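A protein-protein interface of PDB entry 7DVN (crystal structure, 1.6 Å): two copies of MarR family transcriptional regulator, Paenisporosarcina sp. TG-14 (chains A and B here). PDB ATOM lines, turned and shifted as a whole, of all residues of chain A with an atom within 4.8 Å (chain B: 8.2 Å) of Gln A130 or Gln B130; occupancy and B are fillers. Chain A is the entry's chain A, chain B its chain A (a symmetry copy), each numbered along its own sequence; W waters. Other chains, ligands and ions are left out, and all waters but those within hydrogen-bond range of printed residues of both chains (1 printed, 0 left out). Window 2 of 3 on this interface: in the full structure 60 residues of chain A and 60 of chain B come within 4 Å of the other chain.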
ATOM      1  N   GLN A 126       1.299  15.896 -26.755  1.00  0.00           N
ATOM      2  CA  GLN A 126       0.025  15.163 -26.784  1.00  0.00           C
ATOM      3  C   GLN A 126       0.174  13.863 -25.970  1.00  0.00           C
ATOM      4  O   GLN A 126      -0.706  13.518 -25.197  1.00  0.00           O
ATOM      5  CB  GLN A 126      -0.435  14.870 -28.209  1.00  0.00           C
ATOM      6  CG  GLN A 126      -1.845  15.380 -28.470  1.00  0.00           C
ATOM      7  CD  GLN A 126      -2.478  14.878 -29.748  1.00  0.00           C
ATOM      8  OE1 GLN A 126      -2.316  15.603 -30.748  1.00  0.00           O
ATOM      9  NE2 GLN A 126      -3.178  13.722 -29.673  1.00  0.00           N
ATOM     10  N   GLU A 127       1.271  13.138 -26.143  1.00  0.00           N
ATOM     11  CA  GLU A 127       1.471  11.831 -25.485  1.00  0.00           C
ATOM     12  C   GLU A 127       1.648  12.051 -23.970  1.00  0.00           C
ATOM     13  O   GLU A 127       1.094  11.246 -23.183  1.00  0.00           O
ATOM     14  CB  GLU A 127       2.708  11.108 -26.027  1.00  0.00           C
ATOM     15  CG  GLU A 127       2.518  10.516 -27.412  1.00  0.00           C
ATOM     16  CD  GLU A 127       3.831   9.982 -28.019  1.00  0.00           C
ATOM     17  OE1 GLU A 127       4.752  10.784 -28.196  1.00  0.00           O
ATOM     18  OE2 GLU A 127       3.772   8.878 -28.522  1.00  0.00           O
ATOM     19  N   ILE A 128       2.384  13.068 -23.583  1.00  0.00           N
ATOM     20  CA  ILE A 128       2.575  13.365 -22.145  1.00  0.00           C
ATOM     21  C   ILE A 128       1.230  13.696 -21.496  1.00  0.00           C
ATOM     22  O   ILE A 128       0.872  13.158 -20.472  1.00  0.00           O
ATOM     23  CB  ILE A 128       3.621  14.463 -21.969  1.00  0.00           C
ATOM     24  CG1 ILE A 128       4.986  14.010 -22.468  1.00  0.00           C
ATOM     25  CG2 ILE A 128       3.624  14.913 -20.516  1.00  0.00           C
ATOM     26  CD1 ILE A 128       5.954  15.179 -22.666  1.00  0.00           C
ATOM     27  N   GLU A 129       0.467  14.573 -22.137  1.00  0.00           N
ATOM     28  CA  GLU A 129      -0.828  15.006 -21.560  1.00  0.00           C
ATOM     29  C   GLU A 129      -1.775  13.792 -21.498  1.00  0.00           C
ATOM     30  O   GLU A 129      -2.531  13.689 -20.540  1.00  0.00           O
ATOM     31  CB  GLU A 129      -1.483  16.085 -22.419  1.00  0.00           C
ATOM     32  CG  GLU A 129      -0.736  17.394 -22.380  1.00  0.00           C
ATOM     33  CD  GLU A 129      -0.719  18.137 -21.054  1.00  0.00           C
ATOM     34  OE1 GLU A 129      -1.463  17.768 -20.089  1.00  0.00           O
ATOM     35  OE2 GLU A 129       0.073  19.130 -20.980  1.00  0.00           O
ATOM     36  N   GLN A 130      -1.784  12.909 -22.507  1.00  0.00           N
ATOM     37  CA  GLN A 130      -2.636  11.716 -22.472  1.00  0.00           C
ATOM     38  C   GLN A 130      -2.222  10.822 -21.320  1.00  0.00           C
ATOM     39  O   GLN A 130      -3.082  10.276 -20.597  1.00  0.00           O
ATOM     40  CB  GLN A 130      -2.639  10.906 -23.768  1.00  0.00           C
ATOM     41  CG  GLN A 130      -3.497  11.464 -24.874  1.00  0.00           C
ATOM     42  CD  GLN A 130      -3.504  10.481 -26.030  1.00  0.00           C
ATOM     43  OE1 GLN A 130      -2.576  10.460 -26.833  1.00  0.00           O
ATOM     44  NE2 GLN A 130      -4.573   9.711 -26.148  1.00  0.00           N
ATOM     45  N   PHE A 131      -0.916  10.644 -21.148  1.00  0.00           N
ATOM     46  CA  PHE A 131      -0.388   9.791 -20.056  1.00  0.00           C
ATOM     47  C   PHE A 131      -0.904  10.279 -18.686  1.00  0.00           C
ATOM     48  O   PHE A 131      -1.283   9.448 -17.861  1.00  0.00           O
ATOM     49  CB  PHE A 131       1.139   9.763 -20.129  1.00  0.00           C
ATOM     50  CG  PHE A 131       1.864   8.868 -19.139  1.00  0.00           C
ATOM     51  CD1 PHE A 131       2.024   9.252 -17.813  1.00  0.00           C
ATOM     52  CD2 PHE A 131       2.341   7.627 -19.539  1.00  0.00           C
ATOM     53  CE1 PHE A 131       2.662   8.405 -16.919  1.00  0.00           C
ATOM     54  CE2 PHE A 131       3.002   6.795 -18.650  1.00  0.00           C
ATOM     55  CZ  PHE A 131       3.160   7.200 -17.342  1.00  0.00           C
ATOM     56  N   LEU A 132      -0.960  11.598 -18.464  1.00  0.00           N
ATOM     57  CA  LEU A 132      -1.438  12.152 -17.177  1.00  0.00           C
ATOM     58  C   LEU A 132      -2.879  11.713 -16.949  1.00  0.00           C
ATOM     59  O   LEU A 132      -3.203  11.274 -15.906  1.00  0.00           O
ATOM     60  CB  LEU A 132      -1.292  13.663 -17.135  1.00  0.00           C
ATOM     61  CG  LEU A 132       0.130  14.191 -17.293  1.00  0.00           C
ATOM     62  CD1 LEU A 132       0.102  15.694 -17.265  1.00  0.00           C
ATOM     63  CD2 LEU A 132       1.044  13.657 -16.182  1.00  0.00           C
ATOM     64  N   VAL A 133      -3.732  11.801 -17.983  1.00  0.00           N
ATOM     65  CA  VAL A 133      -5.159  11.450 -17.759  1.00  0.00           C
ATOM     66  C   VAL A 133      -5.245   9.945 -17.524  1.00  0.00           C
ATOM     67  O   VAL A 133      -5.934   9.513 -16.580  1.00  0.00           O
ATOM     68  CB  VAL A 133      -5.968  11.890 -18.986  1.00  0.00           C
ATOM     69  CG1 VAL A 133      -7.386  11.347 -18.892  1.00  0.00           C
ATOM     70  CG2 VAL A 133      -5.885  13.386 -19.154  1.00  0.00           C
ATOM     71  N   THR A 134      -4.592   9.113 -18.339  1.00  0.00           N
ATOM     72  CA  THR A 134      -4.619   7.643 -18.236  1.00  0.00           C
ATOM     73  C   THR A 134      -4.143   7.232 -16.827  1.00  0.00           C
ATOM     74  O   THR A 134      -4.779   6.419 -16.175  1.00  0.00           O
ATOM     75  CB  THR A 134      -3.663   7.054 -19.284  1.00  0.00           C
ATOM     76  OG1 THR A 134      -4.146   7.478 -20.567  1.00  0.00           O
ATOM     77  CG2 THR A 134      -3.571   5.551 -19.130  1.00  0.00           C
ATOM     78  N   LEU B  11       3.001   9.880 -10.831  1.00  0.00           N
ATOM     79  CA  LEU B  11       1.840   8.988 -11.048  1.00  0.00           C
ATOM     80  C   LEU B  11       2.286   7.562 -11.294  1.00  0.00           C
ATOM     81  O   LEU B  11       1.631   6.596 -10.865  1.00  0.00           O
ATOM     82  CB  LEU B  11       0.971   9.500 -12.198  1.00  0.00           C
ATOM     83  CG  LEU B  11       0.040  10.657 -11.859  1.00  0.00           C
ATOM     84  CD1 LEU B  11      -0.547  11.278 -13.148  1.00  0.00           C
ATOM     85  CD2 LEU B  11      -1.067  10.237 -10.936  1.00  0.00           C
ATOM     86  N   ASP B 124     -11.706   0.395 -20.982  1.00  0.00           N
ATOM     87  CA  ASP B 124     -12.235  -0.307 -22.170  1.00  0.00           C
ATOM     88  C   ASP B 124     -11.102  -0.863 -23.026  1.00  0.00           C
ATOM     89  O   ASP B 124      -9.890  -0.662 -22.739  1.00  0.00           O
ATOM     90  CB  ASP B 124     -13.197   0.571 -22.949  1.00  0.00           C
ATOM     91  CG  ASP B 124     -12.622   1.856 -23.472  1.00  0.00           C
ATOM     92  OD1 ASP B 124     -11.434   1.876 -23.791  1.00  0.00           O
ATOM     93  OD2 ASP B 124     -13.402   2.857 -23.560  1.00  0.00           O
ATOM     94  N   ASP B 125     -11.492  -1.689 -23.967  1.00  0.00           N
ATOM     95  CA  ASP B 125     -10.536  -2.378 -24.862  1.00  0.00           C
ATOM     96  C   ASP B 125      -9.641  -1.347 -25.520  1.00  0.00           C
ATOM     97  O   ASP B 125      -8.384  -1.585 -25.648  1.00  0.00           O
ATOM     98  CB  ASP B 125     -11.298  -3.169 -25.926  1.00  0.00           C
ATOM     99  CG  ASP B 125     -12.036  -4.346 -25.326  1.00  0.00           C
ATOM    100  OD1 ASP B 125     -11.665  -4.771 -24.211  1.00  0.00           O
ATOM    101  OD2 ASP B 125     -13.013  -4.788 -25.958  1.00  0.00           O
ATOM    102  N   GLN B 126     -10.196  -0.245 -26.006  1.00  0.00           N
ATOM    103  CA  GLN B 126      -9.438   0.823 -26.673  1.00  0.00           C
ATOM    104  C   GLN B 126      -8.298   1.286 -25.745  1.00  0.00           C
ATOM    105  O   GLN B 126      -7.178   1.476 -26.195  1.00  0.00           O
ATOM    106  CB  GLN B 126     -10.331   1.994 -27.075  1.00  0.00           C
ATOM    107  CG  GLN B 126     -10.210   2.321 -28.555  1.00  0.00           C
ATOM    108  CD  GLN B 126     -10.830   3.636 -28.969  1.00  0.00           C
ATOM    109  OE1 GLN B 126     -12.014   3.576 -29.350  1.00  0.00           O
ATOM    110  NE2 GLN B 126     -10.036   4.732 -28.918  1.00  0.00           N
ATOM    111  N   GLU B 127      -8.573   1.477 -24.461  1.00  0.00           N
ATOM    112  CA  GLU B 127      -7.579   2.008 -23.508  1.00  0.00           C
ATOM    113  C   GLU B 127      -6.474   0.956 -23.291  1.00  0.00           C
ATOM    114  O   GLU B 127      -5.285   1.348 -23.219  1.00  0.00           O
ATOM    115  CB  GLU B 127      -8.216   2.341 -22.155  1.00  0.00           C
ATOM    116  CG  GLU B 127      -9.059   3.604 -22.165  1.00  0.00           C
ATOM    117  CD  GLU B 127      -9.854   3.802 -20.858  1.00  0.00           C
ATOM    118  OE1 GLU B 127     -10.675   2.936 -20.548  1.00  0.00           O
ATOM    119  OE2 GLU B 127      -9.808   4.915 -20.373  1.00  0.00           O
ATOM    120  N   ILE B 128      -6.842  -0.301 -23.180  1.00  0.00           N
ATOM    121  CA  ILE B 128      -5.837  -1.373 -23.003  1.00  0.00           C
ATOM    122  C   ILE B 128      -4.913  -1.431 -24.221  1.00  0.00           C
ATOM    123  O   ILE B 128      -3.709  -1.443 -24.101  1.00  0.00           O
ATOM    124  CB  ILE B 128      -6.532  -2.700 -22.704  1.00  0.00           C
ATOM    125  CG1 ILE B 128      -7.289  -2.641 -21.385  1.00  0.00           C
ATOM    126  CG2 ILE B 128      -5.504  -3.820 -22.764  1.00  0.00           C
ATOM    127  CD1 ILE B 128      -8.294  -3.786 -21.236  1.00  0.00           C
ATOM    128  N   GLU B 129      -5.505  -1.429 -25.409  1.00  0.00           N
ATOM    129  CA  GLU B 129      -4.700  -1.543 -26.649  1.00  0.00           C
ATOM    130  C   GLU B 129      -3.799  -0.299 -26.774  1.00  0.00           C
ATOM    131  O   GLU B 129      -2.671  -0.438 -27.228  1.00  0.00           O
ATOM    132  CB  GLU B 129      -5.595  -1.616 -27.885  1.00  0.00           C
ATOM    133  CG  GLU B 129      -6.374  -2.904 -27.965  1.00  0.00           C
ATOM    134  CD  GLU B 129      -5.574  -4.178 -28.188  1.00  0.00           C
ATOM    135  OE1 GLU B 129      -4.338  -4.129 -28.488  1.00  0.00           O
ATOM    136  OE2 GLU B 129      -6.213  -5.269 -28.056  1.00  0.00           O
ATOM    137  N   GLN B 130      -4.282   0.904 -26.429  1.00  0.00           N
ATOM    138  CA  GLN B 130      -3.449   2.109 -26.489  1.00  0.00           C
ATOM    139  C   GLN B 130      -2.291   1.982 -25.519  1.00  0.00           C
ATOM    140  O   GLN B 130      -1.141   2.340 -25.850  1.00  0.00           O
ATOM    141  CB  GLN B 130      -4.202   3.410 -26.215  1.00  0.00           C
ATOM    142  CG  GLN B 130      -5.017   3.937 -27.368  1.00  0.00           C
ATOM    143  CD  GLN B 130      -5.583   5.292 -26.986  1.00  0.00           C
ATOM    144  OE1 GLN B 130      -6.599   5.371 -26.302  1.00  0.00           O
ATOM    145  NE2 GLN B 130      -4.963   6.354 -27.474  1.00  0.00           N
ATOM    146  N   PHE B 131      -2.579   1.498 -24.314  1.00  0.00           N
ATOM    147  CA  PHE B 131      -1.531   1.329 -23.278  1.00  0.00           C
ATOM    148  C   PHE B 131      -0.388   0.434 -23.802  1.00  0.00           C
ATOM    149  O   PHE B 131       0.776   0.754 -23.566  1.00  0.00           O
ATOM    150  CB  PHE B 131      -2.167   0.777 -22.002  1.00  0.00           C
ATOM    151  CG  PHE B 131      -1.263   0.614 -20.791  1.00  0.00           C
ATOM    152  CD1 PHE B 131      -0.375  -0.450 -20.701  1.00  0.00           C
ATOM    153  CD2 PHE B 131      -1.283   1.558 -19.774  1.00  0.00           C
ATOM    154  CE1 PHE B 131       0.463  -0.562 -19.601  1.00  0.00           C
ATOM    155  CE2 PHE B 131      -0.464   1.429 -18.663  1.00  0.00           C
ATOM    156  CZ  PHE B 131       0.401   0.359 -18.588  1.00  0.00           C
ATOM    157  N   LEU B 132      -0.710  -0.641 -24.533  1.00  0.00           N
ATOM    158  CA  LEU B 132       0.323  -1.555 -25.070  1.00  0.00           C
ATOM    159  C   LEU B 132       1.242  -0.777 -26.004  1.00  0.00           C
ATOM    160  O   LEU B 132       2.409  -0.886 -25.907  1.00  0.00           O
ATOM    161  CB  LEU B 132      -0.302  -2.755 -25.760  1.00  0.00           C
ATOM    162  CG  LEU B 132      -1.191  -3.629 -24.882  1.00  0.00           C
ATOM    163  CD1 LEU B 132      -1.758  -4.745 -25.714  1.00  0.00           C
ATOM    164  CD2 LEU B 132      -0.404  -4.200 -23.695  1.00  0.00           C
ATOM    165  N   VAL B 133       0.673   0.058 -26.890  1.00  0.00           N
ATOM    166  CA  VAL B 133       1.548   0.768 -27.860  1.00  0.00           C
ATOM    167  C   VAL B 133       2.379   1.789 -27.089  1.00  0.00           C
ATOM    168  O   VAL B 133       3.602   1.874 -27.312  1.00  0.00           O
ATOM    169  CB  VAL B 133       0.662   1.429 -28.923  1.00  0.00           C
ATOM    170  CG1 VAL B 133       1.502   2.347 -29.799  1.00  0.00           C
ATOM    171  CG2 VAL B 133      -0.109   0.380 -29.683  1.00  0.00           C
ATOM    172  N   THR B 134       1.783   2.585 -26.197  1.00  0.00           N
ATOM    173  CA  THR B 134       2.467   3.627 -25.413  1.00  0.00           C
ATOM    174  C   THR B 134       3.621   2.979 -24.620  1.00  0.00           C
ATOM    175  O   THR B 134       4.734   3.484 -24.628  1.00  0.00           O
ATOM    176  CB  THR B 134       1.464   4.248 -24.429  1.00  0.00           C
ATOM    177  OG1 THR B 134       0.411   4.820 -25.219  1.00  0.00           O
ATOM    178  CG2 THR B 134       2.157   5.240 -23.521  1.00  0.00           C
ATOM    179  N   PHE B 135       3.342   1.869 -23.951  1.00  0.00           N
ATOM    180  CA  PHE B 135       4.338   1.245 -23.047  1.00  0.00           C
ATOM    181  C   PHE B 135       5.447   0.539 -23.835  1.00  0.00           C
ATOM    182  O   PHE B 135       6.585   0.506 -23.348  1.00  0.00           O
ATOM    183  CB  PHE B 135       3.639   0.377 -21.999  1.00  0.00           C
ATOM    184  CG  PHE B 135       3.478   1.204 -20.748  1.00  0.00           C
ATOM    185  CD1 PHE B 135       2.608   2.277 -20.707  1.00  0.00           C
ATOM    186  CD2 PHE B 135       4.253   0.955 -19.622  1.00  0.00           C
ATOM    187  CE1 PHE B 135       2.561   3.113 -19.613  1.00  0.00           C
ATOM    188  CE2 PHE B 135       4.203   1.806 -18.531  1.00  0.00           C
ATOM    189  CZ  PHE B 135       3.375   2.906 -18.535  1.00  0.00           C
ATOM    190  N   ARG B 136       5.123  -0.057 -24.989  1.00  0.00           N
ATOM    191  CA  ARG B 136       6.243  -0.601 -25.814  1.00  0.00           C
ATOM    192  C   ARG B 136       7.174   0.546 -26.182  1.00  0.00           C
ATOM    193  O   ARG B 136       8.415   0.357 -26.167  1.00  0.00           O
ATOM    194  CB  ARG B 136       5.785  -1.389 -27.020  1.00  0.00           C
ATOM    195  CG  ARG B 136       5.077  -2.689 -26.669  1.00  0.00           C
ATOM    196  CD  ARG B 136       5.050  -3.583 -27.885  1.00  0.00           C
ATOM    197  NE  ARG B 136       4.074  -3.063 -28.804  1.00  0.00           N
ATOM    198  CZ  ARG B 136       2.806  -3.442 -28.918  1.00  0.00           C
ATOM    199  NH1 ARG B 136       2.280  -4.343 -28.152  1.00  0.00           N
ATOM    200  NH2 ARG B 136       2.050  -2.920 -29.842  1.00  0.00           N
ATOM    201  N   LYS B 137       6.600   1.690 -26.563  1.00  0.00           N
ATOM    202  CA  LYS B 137       7.425   2.853 -26.944  1.00  0.00           C
ATOM    203  C   LYS B 137       8.265   3.324 -25.763  1.00  0.00           C
ATOM    204  O   LYS B 137       9.458   3.559 -25.924  1.00  0.00           O
ATOM    205  CB  LYS B 137       6.544   3.929 -27.571  1.00  0.00           C
ATOM    206  CG  LYS B 137       7.233   5.245 -27.846  1.00  0.00           C
ATOM    207  CD  LYS B 137       6.330   6.185 -28.610  1.00  0.00           C
ATOM    208  CE  LYS B 137       7.063   7.473 -28.890  1.00  0.00           C
ATOM    209  NZ  LYS B 137       6.249   8.400 -29.706  1.00  0.00           N
HETATM  210  O   HOH W   1       6.414  11.038 -30.674  1.00  0.00           O
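The side-chain carboxylate (OE2) of Glu A127 lies within salt-bridge range of the side-chain amino group (NZ) of Lys B137, at 2.8 Å.
The backbone carbonyl oxygen (O) of Gln B130 sits at hydrogen-bond distance from the side-chain hydroxyl (OG1) of Thr B134, at 3.0 Å.
The backbone carbonyl oxygen of Gln A130 lies within hydrogen-bond range of the side-chain hydroxyl of Thr A134, 3.0 Å away.
Among the printed residues, merely in contact across the chains: Gln A130 with Gln B130 (3.6 Å), Phe A131 with Phe B135 (3.8 Å) and Leu A132 with Leu B11 (3.8 Å).
Printed residues of chain B within 4 Å of Phe A131: Phe B135.
Of the printed residues of chain B, Leu A132 touches Leu B11.
Printed residues of chain A within 4 Å of Leu B11: Leu A132.
Gln B130 touches just one residue of chain A: Gln A130 (3.6 Å).
Printed residues of chain A within 4 Å of Phe B135: Phe A131 (3.8 Å).
Printed residues of chain A within 4 Å of Lys B137: Glu A127.
The nearest printed residue of chain A that does not touch Gln B130 is Thr A134 (6.6 Å).
The nearest printed residue of chain B that does not touch Phe A131 is Thr B134 (4.6 Å).
Of the 9 printed residues of chain A, 4 touch a printed residue of chain B.
Printed residues of chain A that touch a printed residue of chain B: Glu A127, Gln A130, Phe A131 and Leu A132.
Hydrophobic or aromatic side chains of chain A within 4 Å of the printed part of chain B: Phe A131.
Along chain A the printed residues that touch a printed residue of chain B span positions 127 to 132.
Of the 15 printed residues of chain B, 4 touch a printed residue of chain A.
Along chain B the printed residues that touch a printed residue of chain A span positions 11 to 137.
Among the printed residues, Asp or Glu carboxylates within 4 Å of a Lys or Arg side-chain nitrogen of the other chain: Glu A127 with Lys B137.
Gln A130 touches its own counterpart, Gln B130.
Positions printed for both chains: 126, 127, 128, 129, 130, 131, 132, 133 and 134.
Of the 4 pairs that touch across the chains among the printed residues, 1 has its exchanged pair printed and touching as well.
Water W1 bridges NZ of Lys B137 (2.8 Å) and OE1 of Glu A127 (3.0 Å).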
